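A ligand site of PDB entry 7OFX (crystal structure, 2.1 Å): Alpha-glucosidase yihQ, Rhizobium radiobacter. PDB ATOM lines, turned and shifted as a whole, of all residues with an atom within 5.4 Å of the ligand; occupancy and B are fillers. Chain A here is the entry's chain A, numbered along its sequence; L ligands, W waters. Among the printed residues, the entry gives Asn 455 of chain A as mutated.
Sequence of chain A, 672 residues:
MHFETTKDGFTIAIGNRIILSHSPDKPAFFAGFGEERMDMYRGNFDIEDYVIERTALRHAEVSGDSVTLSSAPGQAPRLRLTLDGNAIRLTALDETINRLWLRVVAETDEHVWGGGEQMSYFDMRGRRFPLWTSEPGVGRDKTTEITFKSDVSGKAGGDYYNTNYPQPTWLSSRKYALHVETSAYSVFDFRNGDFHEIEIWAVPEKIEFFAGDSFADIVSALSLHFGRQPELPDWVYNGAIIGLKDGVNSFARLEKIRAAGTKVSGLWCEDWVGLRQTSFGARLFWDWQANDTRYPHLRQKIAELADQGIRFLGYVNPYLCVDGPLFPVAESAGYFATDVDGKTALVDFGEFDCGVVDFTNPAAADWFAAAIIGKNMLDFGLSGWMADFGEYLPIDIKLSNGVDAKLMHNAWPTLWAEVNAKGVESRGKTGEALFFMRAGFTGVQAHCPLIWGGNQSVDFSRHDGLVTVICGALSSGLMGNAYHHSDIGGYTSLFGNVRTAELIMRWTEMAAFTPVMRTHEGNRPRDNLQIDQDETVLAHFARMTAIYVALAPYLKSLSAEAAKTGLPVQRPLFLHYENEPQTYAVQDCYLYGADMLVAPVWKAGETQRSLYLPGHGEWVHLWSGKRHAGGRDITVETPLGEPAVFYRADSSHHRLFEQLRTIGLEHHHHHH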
ATOM      1  N   ARG A  42      34.417 -27.924  24.461  1.00  0.00           N
ATOM      2  CA  ARG A  42      33.880 -26.743  25.197  1.00  0.00           C
ATOM      3  C   ARG A  42      34.147 -25.482  24.384  1.00  0.00           C
ATOM      4  O   ARG A  42      34.562 -24.456  24.972  1.00  0.00           O
ATOM      5  CB  ARG A  42      34.499 -26.692  26.599  1.00  0.00           C
ATOM      6  CG  ARG A  42      34.145 -27.928  27.412  1.00  0.00           C
ATOM      7  CD  ARG A  42      34.842 -28.022  28.751  1.00  0.00           C
ATOM      8  NE  ARG A  42      34.413 -29.207  29.489  1.00  0.00           N
ATOM      9  CZ  ARG A  42      34.800 -29.491  30.746  1.00  0.00           C
ATOM     10  NH1 ARG A  42      35.606 -28.672  31.389  1.00  0.00           N
ATOM     11  NH2 ARG A  42      34.363 -30.582  31.349  1.00  0.00           N
ATOM     12  N   GLU A 135      35.522 -20.246  20.908  1.00  0.00           N
ATOM     13  CA  GLU A 135      36.211 -19.637  22.078  1.00  0.00           C
ATOM     14  C   GLU A 135      37.503 -19.014  21.543  1.00  0.00           C
ATOM     15  O   GLU A 135      38.233 -19.604  20.762  1.00  0.00           O
ATOM     16  CB  GLU A 135      36.422 -20.679  23.162  1.00  0.00           C
ATOM     17  CG  GLU A 135      35.133 -20.994  23.932  1.00  0.00           C
ATOM     18  CD  GLU A 135      34.590 -19.886  24.852  1.00  0.00           C
ATOM     19  OE1 GLU A 135      35.288 -18.900  25.050  1.00  0.00           O
ATOM     20  OE2 GLU A 135      33.435 -20.011  25.344  1.00  0.00           O
ATOM     21  N   LYS A 245      25.697  -9.922  39.806  1.00  0.00           N
ATOM     22  CA  LYS A 245      25.091 -11.277  39.722  1.00  0.00           C
ATOM     23  C   LYS A 245      24.975 -11.805  41.145  1.00  0.00           C
ATOM     24  O   LYS A 245      25.318 -12.979  41.379  1.00  0.00           O
ATOM     25  CB  LYS A 245      25.912 -12.111  38.734  1.00  0.00           C
ATOM     26  CG  LYS A 245      27.423 -12.081  38.971  1.00  0.00           C
ATOM     27  CD  LYS A 245      28.212 -12.730  37.879  1.00  0.00           C
ATOM     28  CE  LYS A 245      28.091 -14.237  37.828  1.00  0.00           C
ATOM     29  NZ  LYS A 245      28.859 -14.786  36.678  1.00  0.00           N
ATOM     30  N   TRP A 268      22.306  -4.567  35.072  1.00  0.00           N
ATOM     31  CA  TRP A 268      22.401  -5.796  34.246  1.00  0.00           C
ATOM     32  C   TRP A 268      22.693  -6.974  35.178  1.00  0.00           C
ATOM     33  O   TRP A 268      23.776  -6.993  35.802  1.00  0.00           O
ATOM     34  CB  TRP A 268      23.447  -5.633  33.149  1.00  0.00           C
ATOM     35  CG  TRP A 268      23.784  -6.911  32.476  1.00  0.00           C
ATOM     36  CD1 TRP A 268      22.931  -7.753  31.834  1.00  0.00           C
ATOM     37  CD2 TRP A 268      25.074  -7.526  32.418  1.00  0.00           C
ATOM     38  NE1 TRP A 268      23.605  -8.852  31.354  1.00  0.00           N
ATOM     39  CE2 TRP A 268      24.911  -8.751  31.729  1.00  0.00           C
ATOM     40  CE3 TRP A 268      26.333  -7.154  32.887  1.00  0.00           C
ATOM     41  CZ2 TRP A 268      25.969  -9.624  31.507  1.00  0.00           C
ATOM     42  CZ3 TRP A 268      27.380  -8.021  32.672  1.00  0.00           C
ATOM     43  CH2 TRP A 268      27.196  -9.226  31.977  1.00  0.00           C
ATOM     44  N   GLU A 270      22.888 -10.836  34.985  1.00  0.00           N
ATOM     45  CA  GLU A 270      22.924 -12.040  34.102  1.00  0.00           C
ATOM     46  C   GLU A 270      22.382 -13.232  34.898  1.00  0.00           C
ATOM     47  O   GLU A 270      21.890 -14.179  34.223  1.00  0.00           O
ATOM     48  CB  GLU A 270      24.340 -12.264  33.543  1.00  0.00           C
ATOM     49  CG  GLU A 270      25.406 -12.602  34.566  1.00  0.00           C
ATOM     50  CD  GLU A 270      26.726 -13.096  33.986  1.00  0.00           C
ATOM     51  OE1 GLU A 270      27.612 -13.474  34.809  1.00  0.00           O
ATOM     52  OE2 GLU A 270      26.870 -13.154  32.756  1.00  0.00           O
ATOM     53  N   PHE A 280      34.676 -23.884  36.916  1.00  0.00           N
ATOM     54  CA  PHE A 280      34.982 -22.616  36.204  1.00  0.00           C
ATOM     55  C   PHE A 280      34.636 -21.397  37.100  1.00  0.00           C
ATOM     56  O   PHE A 280      35.413 -20.424  37.145  1.00  0.00           O
ATOM     57  CB  PHE A 280      34.257 -22.570  34.860  1.00  0.00           C
ATOM     58  CG  PHE A 280      34.591 -21.362  34.022  1.00  0.00           C
ATOM     59  CD1 PHE A 280      35.739 -21.333  33.246  1.00  0.00           C
ATOM     60  CD2 PHE A 280      33.716 -20.271  33.978  1.00  0.00           C
ATOM     61  CE1 PHE A 280      36.011 -20.238  32.429  1.00  0.00           C
ATOM     62  CE2 PHE A 280      34.001 -19.176  33.167  1.00  0.00           C
ATOM     63  CZ  PHE A 280      35.147 -19.157  32.411  1.00  0.00           C
ATOM     64  N   ALA A 282      31.087 -19.156  39.171  1.00  0.00           N
ATOM     65  CA  ALA A 282      29.640 -18.852  39.290  1.00  0.00           C
ATOM     66  C   ALA A 282      29.041 -18.684  37.889  1.00  0.00           C
ATOM     67  O   ALA A 282      28.919 -17.534  37.447  1.00  0.00           O
ATOM     68  CB  ALA A 282      29.462 -17.619  40.141  1.00  0.00           C
ATOM     69  N   ARG A 283      28.687 -19.779  37.238  1.00  0.00           N
ATOM     70  CA  ARG A 283      28.049 -19.720  35.907  1.00  0.00           C
ATOM     71  C   ARG A 283      26.531 -19.569  36.082  1.00  0.00           C
ATOM     72  O   ARG A 283      26.067 -19.475  37.247  1.00  0.00           O
ATOM     73  CB  ARG A 283      28.471 -20.932  35.083  1.00  0.00           C
ATOM     74  CG  ARG A 283      29.980 -20.992  34.875  1.00  0.00           C
ATOM     75  CD  ARG A 283      30.376 -21.982  33.797  1.00  0.00           C
ATOM     76  NE  ARG A 283      30.045 -21.517  32.467  1.00  0.00           N
ATOM     77  CZ  ARG A 283      30.376 -22.146  31.351  1.00  0.00           C
ATOM     78  NH1 ARG A 283      30.994 -23.318  31.398  1.00  0.00           N
ATOM     79  NH2 ARG A 283      30.038 -21.646  30.185  1.00  0.00           N
ATOM     80  N   LEU A 284      25.795 -19.535  34.979  1.00  0.00           N
ATOM     81  CA  LEU A 284      24.334 -19.276  34.996  1.00  0.00           C
ATOM     82  C   LEU A 284      23.567 -20.567  34.719  1.00  0.00           C
ATOM     83  O   LEU A 284      24.135 -21.509  34.112  1.00  0.00           O
ATOM     84  CB  LEU A 284      24.054 -18.207  33.940  1.00  0.00           C
ATOM     85  CG  LEU A 284      24.849 -16.915  34.056  1.00  0.00           C
ATOM     86  CD1 LEU A 284      24.400 -15.943  32.981  1.00  0.00           C
ATOM     87  CD2 LEU A 284      24.713 -16.297  35.438  1.00  0.00           C
ATOM     88  N   TRP A 286      21.034 -22.188  32.498  1.00  0.00           N
ATOM     89  CA  TRP A 286      20.607 -21.875  31.108  1.00  0.00           C
ATOM     90  C   TRP A 286      19.173 -22.349  30.851  1.00  0.00           C
ATOM     91  O   TRP A 286      18.933 -23.337  30.119  1.00  0.00           O
ATOM     92  CB  TRP A 286      21.592 -22.486  30.128  1.00  0.00           C
ATOM     93  CG  TRP A 286      22.964 -21.892  30.214  1.00  0.00           C
ATOM     94  CD1 TRP A 286      23.439 -20.983  31.113  1.00  0.00           C
ATOM     95  CD2 TRP A 286      24.058 -22.191  29.344  1.00  0.00           C
ATOM     96  NE1 TRP A 286      24.743 -20.682  30.849  1.00  0.00           N
ATOM     97  CE2 TRP A 286      25.153 -21.409  29.767  1.00  0.00           C
ATOM     98  CE3 TRP A 286      24.204 -23.027  28.247  1.00  0.00           C
ATOM     99  CZ2 TRP A 286      26.389 -21.439  29.138  1.00  0.00           C
ATOM    100  CZ3 TRP A 286      25.438 -23.091  27.641  1.00  0.00           C
ATOM    101  CH2 TRP A 286      26.515 -22.315  28.070  1.00  0.00           C
ATOM    102  N   TYR A 315      20.109 -11.691  30.298  1.00  0.00           N
ATOM    103  CA  TYR A 315      21.065 -12.632  29.660  1.00  0.00           C
ATOM    104  C   TYR A 315      20.269 -13.735  29.003  1.00  0.00           C
ATOM    105  O   TYR A 315      19.312 -14.222  29.601  1.00  0.00           O
ATOM    106  CB  TYR A 315      21.988 -13.252  30.712  1.00  0.00           C
ATOM    107  CG  TYR A 315      22.958 -14.249  30.129  1.00  0.00           C
ATOM    108  CD1 TYR A 315      22.540 -15.531  29.806  1.00  0.00           C
ATOM    109  CD2 TYR A 315      24.267 -13.908  29.854  1.00  0.00           C
ATOM    110  CE1 TYR A 315      23.408 -16.445  29.239  1.00  0.00           C
ATOM    111  CE2 TYR A 315      25.162 -14.813  29.278  1.00  0.00           C
ATOM    112  CZ  TYR A 315      24.718 -16.080  28.960  1.00  0.00           C
ATOM    113  OH  TYR A 315      25.579 -16.992  28.408  1.00  0.00           O
ATOM    114  N   PHE A 352      28.183 -29.528  32.487  1.00  0.00           N
ATOM    115  CA  PHE A 352      26.722 -29.611  32.244  1.00  0.00           C
ATOM    116  C   PHE A 352      26.474 -29.740  30.733  1.00  0.00           C
ATOM    117  O   PHE A 352      27.313 -29.260  29.920  1.00  0.00           O
ATOM    118  CB  PHE A 352      25.992 -28.410  32.842  1.00  0.00           C
ATOM    119  CG  PHE A 352      26.395 -27.062  32.323  1.00  0.00           C
ATOM    120  CD1 PHE A 352      27.526 -26.403  32.789  1.00  0.00           C
ATOM    121  CD2 PHE A 352      25.625 -26.411  31.376  1.00  0.00           C
ATOM    122  CE1 PHE A 352      27.849 -25.140  32.343  1.00  0.00           C
ATOM    123  CE2 PHE A 352      25.987 -25.158  30.898  1.00  0.00           C
ATOM    124  CZ  PHE A 352      27.097 -24.521  31.377  1.00  0.00           C
ATOM    125  N   MET A 386      22.670  -9.291  27.403  1.00  0.00           N
ATOM    126  CA  MET A 386      23.755 -10.051  26.750  1.00  0.00           C
ATOM    127  C   MET A 386      23.107 -11.180  25.929  1.00  0.00           C
ATOM    128  O   MET A 386      22.363 -11.994  26.512  1.00  0.00           O
ATOM    129  CB  MET A 386      24.704 -10.599  27.829  1.00  0.00           C
ATOM    130  CG  MET A 386      25.879 -11.380  27.267  1.00  0.00           C
ATOM    131  SD  MET A 386      27.040 -11.713  28.571  1.00  0.00           S
ATOM    132  CE  MET A 386      27.959 -10.189  28.683  1.00  0.00           C
ATOM    133  N   ASP A 388      24.440 -14.146  24.184  1.00  0.00           N
ATOM    134  CA  ASP A 388      25.768 -14.773  24.345  1.00  0.00           C
ATOM    135  C   ASP A 388      25.920 -15.955  23.397  1.00  0.00           C
ATOM    136  O   ASP A 388      24.910 -16.438  22.849  1.00  0.00           O
ATOM    137  CB  ASP A 388      25.956 -15.207  25.784  1.00  0.00           C
ATOM    138  CG  ASP A 388      27.399 -15.394  26.191  1.00  0.00           C
ATOM    139  OD1 ASP A 388      28.290 -15.051  25.387  1.00  0.00           O
ATOM    140  OD2 ASP A 388      27.619 -15.872  27.325  1.00  0.00           O
ATOM    141  N   PHE A 389      27.150 -16.418  23.247  1.00  0.00           N
ATOM    142  CA  PHE A 389      27.498 -17.683  22.551  1.00  0.00           C
ATOM    143  C   PHE A 389      27.111 -17.582  21.080  1.00  0.00           C
ATOM    144  O   PHE A 389      26.981 -16.475  20.557  1.00  0.00           O
ATOM    145  CB  PHE A 389      26.897 -18.869  23.306  1.00  0.00           C
ATOM    146  CG  PHE A 389      27.594 -19.180  24.602  1.00  0.00           C
ATOM    147  CD1 PHE A 389      28.686 -20.033  24.625  1.00  0.00           C
ATOM    148  CD2 PHE A 389      27.178 -18.600  25.783  1.00  0.00           C
ATOM    149  CE1 PHE A 389      29.333 -20.321  25.824  1.00  0.00           C
ATOM    150  CE2 PHE A 389      27.847 -18.866  26.968  1.00  0.00           C
ATOM    151  CZ  PHE A 389      28.921 -19.726  26.997  1.00  0.00           C
ATOM    152  N   TYR A 392      29.550 -22.587  19.260  1.00  0.00           N
ATOM    153  CA  TYR A 392      29.798 -23.961  19.739  1.00  0.00           C
ATOM    154  C   TYR A 392      29.169 -25.027  18.839  1.00  0.00           C
ATOM    155  O   TYR A 392      28.965 -26.144  19.343  1.00  0.00           O
ATOM    156  CB  TYR A 392      29.281 -24.152  21.158  1.00  0.00           C
ATOM    157  CG  TYR A 392      30.164 -23.658  22.282  1.00  0.00           C
ATOM    158  CD1 TYR A 392      30.598 -22.340  22.336  1.00  0.00           C
ATOM    159  CD2 TYR A 392      30.445 -24.483  23.345  1.00  0.00           C
ATOM    160  CE1 TYR A 392      31.359 -21.893  23.404  1.00  0.00           C
ATOM    161  CE2 TYR A 392      31.190 -24.037  24.432  1.00  0.00           C
ATOM    162  CZ  TYR A 392      31.659 -22.745  24.461  1.00  0.00           C
ATOM    163  OH  TYR A 392      32.393 -22.341  25.537  1.00  0.00           O
ATOM    164  N   ARG A 438      28.862 -11.178  21.428  1.00  0.00           N
ATOM    165  CA  ARG A 438      30.328 -11.404  21.317  1.00  0.00           C
ATOM    166  C   ARG A 438      30.638 -12.193  20.051  1.00  0.00           C
ATOM    167  O   ARG A 438      31.744 -12.016  19.495  1.00  0.00           O
ATOM    168  CB  ARG A 438      30.894 -12.123  22.535  1.00  0.00           C
ATOM    169  CG  ARG A 438      30.434 -13.566  22.644  1.00  0.00           C
ATOM    170  CD  ARG A 438      30.965 -14.260  23.886  1.00  0.00           C
ATOM    171  NE  ARG A 438      30.943 -15.716  23.673  1.00  0.00           N
ATOM    172  CZ  ARG A 438      31.337 -16.604  24.561  1.00  0.00           C
ATOM    173  NH1 ARG A 438      31.326 -17.882  24.234  1.00  0.00           N
ATOM    174  NH2 ARG A 438      31.737 -16.216  25.754  1.00  0.00           N
ATOM    175  N   TRP A 452      30.176  -6.681  21.880  1.00  0.00           N
ATOM    176  CA  TRP A 452      31.153  -6.601  22.999  1.00  0.00           C
ATOM    177  C   TRP A 452      32.328  -7.536  22.727  1.00  0.00           C
ATOM    178  O   TRP A 452      32.148  -8.517  21.983  1.00  0.00           O
ATOM    179  CB  TRP A 452      30.480  -6.770  24.368  1.00  0.00           C
ATOM    180  CG  TRP A 452      30.688  -8.066  25.099  1.00  0.00           C
ATOM    181  CD1 TRP A 452      31.608  -8.316  26.078  1.00  0.00           C
ATOM    182  CD2 TRP A 452      29.848  -9.215  25.041  1.00  0.00           C
ATOM    183  NE1 TRP A 452      31.428  -9.572  26.602  1.00  0.00           N
ATOM    184  CE2 TRP A 452      30.350 -10.153  25.968  1.00  0.00           C
ATOM    185  CE3 TRP A 452      28.715  -9.563  24.285  1.00  0.00           C
ATOM    186  CZ2 TRP A 452      29.798 -11.418  26.134  1.00  0.00           C
ATOM    187  CZ3 TRP A 452      28.168 -10.822  24.440  1.00  0.00           C
ATOM    188  CH2 TRP A 452      28.718 -11.728  25.345  1.00  0.00           C
ATOM    189  N   GLY A 454      33.830  -9.821  24.125  1.00  0.00           N
ATOM    190  CA  GLY A 454      33.845 -11.164  24.716  1.00  0.00           C
ATOM    191  C   GLY A 454      34.609 -11.163  26.026  1.00  0.00           C
ATOM    192  O   GLY A 454      34.569 -10.151  26.738  1.00  0.00           O
ATOM    193  N   ASN A 455      35.285 -12.264  26.313  1.00  0.00           N
ATOM    194  CA  ASN A 455      36.040 -12.497  27.566  1.00  0.00           C
ATOM    195  C   ASN A 455      37.501 -12.102  27.347  1.00  0.00           C
ATOM    196  O   ASN A 455      38.184 -12.748  26.566  1.00  0.00           O
ATOM    197  CB  ASN A 455      35.922 -13.960  28.012  1.00  0.00           C
ATOM    198  CG  ASN A 455      34.496 -14.329  28.339  1.00  0.00           C
ATOM    199  OD1 ASN A 455      33.663 -13.452  28.614  1.00  0.00           O
ATOM    200  ND2 ASN A 455      34.175 -15.615  28.294  1.00  0.00           N
ATOM    201  N   ASP A 487      33.710  -5.523  28.860  1.00  0.00           N
ATOM    202  CA  ASP A 487      33.524  -5.613  30.321  1.00  0.00           C
ATOM    203  C   ASP A 487      34.598  -4.746  30.991  1.00  0.00           C
ATOM    204  O   ASP A 487      35.794  -5.037  30.791  1.00  0.00           O
ATOM    205  CB  ASP A 487      33.742  -7.046  30.815  1.00  0.00           C
ATOM    206  CG  ASP A 487      32.972  -8.112  30.068  1.00  0.00           C
ATOM    207  OD1 ASP A 487      31.784  -7.867  29.732  1.00  0.00           O
ATOM    208  OD2 ASP A 487      33.570  -9.161  29.834  1.00  0.00           O
ATOM    209  N   TYR A 491      36.975 -10.209  32.236  1.00  0.00           N
ATOM    210  CA  TYR A 491      36.069 -11.322  32.657  1.00  0.00           C
ATOM    211  C   TYR A 491      36.839 -12.462  33.348  1.00  0.00           C
ATOM    212  O   TYR A 491      36.478 -12.827  34.488  1.00  0.00           O
ATOM    213  CB  TYR A 491      35.316 -11.856  31.439  1.00  0.00           C
ATOM    214  CG  TYR A 491      34.420 -13.009  31.806  1.00  0.00           C
ATOM    215  CD1 TYR A 491      33.200 -12.801  32.446  1.00  0.00           C
ATOM    216  CD2 TYR A 491      34.846 -14.311  31.648  1.00  0.00           C
ATOM    217  CE1 TYR A 491      32.413 -13.866  32.843  1.00  0.00           C
ATOM    218  CE2 TYR A 491      34.059 -15.387  31.996  1.00  0.00           C
ATOM    219  CZ  TYR A 491      32.851 -15.160  32.626  1.00  0.00           C
ATOM    220  OH  TYR A 491      32.092 -16.230  32.998  1.00  0.00           O
ATOM    221  N   HIS A 520      31.025  -5.950  34.972  1.00  0.00           N
ATOM    222  CA  HIS A 520      30.813  -7.424  34.950  1.00  0.00           C
ATOM    223  C   HIS A 520      31.516  -7.953  36.188  1.00  0.00           C
ATOM    224  O   HIS A 520      32.687  -7.593  36.393  1.00  0.00           O
ATOM    225  CB  HIS A 520      31.354  -8.022  33.651  1.00  0.00           C
ATOM    226  CG  HIS A 520      30.824  -9.370  33.319  1.00  0.00           C
ATOM    227  ND1 HIS A 520      30.384 -10.237  34.291  1.00  0.00           N
ATOM    228  CD2 HIS A 520      30.660 -10.027  32.145  1.00  0.00           C
ATOM    229  CE1 HIS A 520      29.949 -11.369  33.730  1.00  0.00           C
ATOM    230  NE2 HIS A 520      30.105 -11.267  32.402  1.00  0.00           N
HETATM  231  C1  LIG L   1      31.589 -18.036  29.230  1.00  0.00           C
HETATM  232  C2  LIG L   1      32.923 -18.540  28.756  1.00  0.00           C
HETATM  233  C3  LIG L   1      33.129 -20.000  29.108  1.00  0.00           C
HETATM  234  C4  LIG L   1      30.137 -14.702  28.484  1.00  0.00           C
HETATM  235  C5  LIG L   1      30.119 -14.133  29.935  1.00  0.00           C
HETATM  236  C6  LIG L   1      27.833 -16.911  31.359  1.00  0.00           C
HETATM  237  C7  LIG L   1      29.031 -16.259  30.692  1.00  0.00           C
HETATM  238  C8  LIG L   1      30.171 -16.225  28.521  1.00  0.00           C
HETATM  239  C9  LIG L   1      28.938 -14.738  30.680  1.00  0.00           C
HETATM  240  O1  LIG L   1      28.940 -18.621  32.951  1.00  0.00           O
HETATM  241  S1  LIG L   1      28.022 -18.598  31.855  1.00  0.00           S
HETATM  242  O2  LIG L   1      28.406 -19.394  30.715  1.00  0.00           O
HETATM  243  O3  LIG L   1      26.641 -18.958  32.235  1.00  0.00           O
HETATM  244  O4  LIG L   1      29.153 -16.776  29.352  1.00  0.00           O
HETATM  245  O5  LIG L   1      31.428 -16.617  29.016  1.00  0.00           O
HETATM  246  O6  LIG L   1      32.959 -18.361  27.347  1.00  0.00           O
HETATM  247  O7  LIG L   1      34.212 -20.554  28.370  1.00  0.00           O
HETATM  248  O8  LIG L   1      31.222 -14.234  27.698  1.00  0.00           O
HETATM  249  O9  LIG L   1      29.987 -12.705  30.010  1.00  0.00           O
HETATM  250  O10 LIG L   1      28.936 -14.281  32.015  1.00  0.00           O
HETATM  251  O   HOH W   1      34.598 -23.167  27.427  1.00  0.00           O
HETATM  252  O   HOH W   2      29.823 -16.069  34.135  1.00  0.00           O
HETATM  253  O   HOH W   3      31.993 -11.054  28.902  1.00  0.00           O
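An oxygen (O3) of the ligand sits at hydrogen-bond distance from the backbone NH (N) of Leu 284 (2.9 Å).
O3 of the ligand is in hydrogen-bond range of NE1 of Trp 286, at 2.9 Å.
An oxygen (O9) of the ligand is in hydrogen-bond range of a ring nitrogen (NE2) of His 520.
The side-chain carboxylate (OE2) of Glu 135 lies within hydrogen-bond range of an oxygen (O6) of the ligand, 2.6 Å away.
The side-chain carboxylate (OE2) of Glu 270 is in hydrogen-bond range of an oxygen (O10) of the ligand.
O2 of the ligand is in salt-bridge range of NH2 of Arg 283 (2.8 Å).
OD2 of Asp 388 sits close to O4 of the ligand (2.7 Å).
O9 of the ligand sits at hydrogen-bond distance from SD of Met 386.
The guanidinium group (NH2) of Arg 438 is in hydrogen-bond range of an oxygen (O8) of the ligand, 2.8 Å away.
An oxygen (O8) of the ligand is in hydrogen-bond range of the side-chain amide oxygen (OD1) of Asn 455 (2.7 Å).
The backbone carbonyl oxygen (O) of Leu 284 lies close to the indole nitrogen (NE1) of Trp 286 (3.4 Å).
The guanidinium group (NH1) of Arg 438 is in salt-bridge range of the side-chain carboxylate (OE2) of Glu 135 (3.2 Å).
OD1 of Asp 388 lies within salt-bridge range of NE of Arg 438, at 3.2 Å.
OH of Tyr 392 sits at hydrogen-bond distance from OE2 of Glu 135, 2.6 Å away.
OD2 of Asp 388 is in hydrogen-bond range of OH of Tyr 315.
The side-chain amino group (NZ) of Lys 245 is in salt-bridge range of the side-chain carboxylate (OE1) of Glu 270 (2.6 Å).
The indole nitrogen (NE1) of Trp 452 lies within hydrogen-bond range of the backbone carbonyl oxygen (O) of Gly 454 (3.2 Å).
OH of Tyr 392 lies within hydrogen-bond range of O of Arg 42, 3.1 Å away.
Phe 280 touches the ligand.
OH of Tyr 315 touches O4 of the ligand, 3.7 Å away.
CE2 of Phe 389 touches O4 of the ligand (3.4 Å).
Tyr 392 touches the ligand (OH to O7, 3.8 Å).
Trp 452 touches the ligand.
Tyr 491 touches the ligand.
16 residues have an atom within 4 Å of the ligand: Glu 135, Glu 270, Phe 280, Arg 283, Leu 284, Trp 286, Tyr 315, Met 386, Asp 388, Phe 389, Tyr 392, Arg 438, Trp 452, Asn 455, Tyr 491 and His 520.
Along chain A the residues within 4 Å of the ligand span positions 135 to 520.
Water W1 lies within hydrogen-bond range of O of Arg 42, O7 of the ligand and OH of Tyr 392.
Water W2 lies within hydrogen-bond range of OH of Tyr 491 (2.5 Å), O10 of the ligand (2.9 Å), NZ of Lys 245 (3.0 Å) and OE1 of Glu 270 (3.5 Å).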
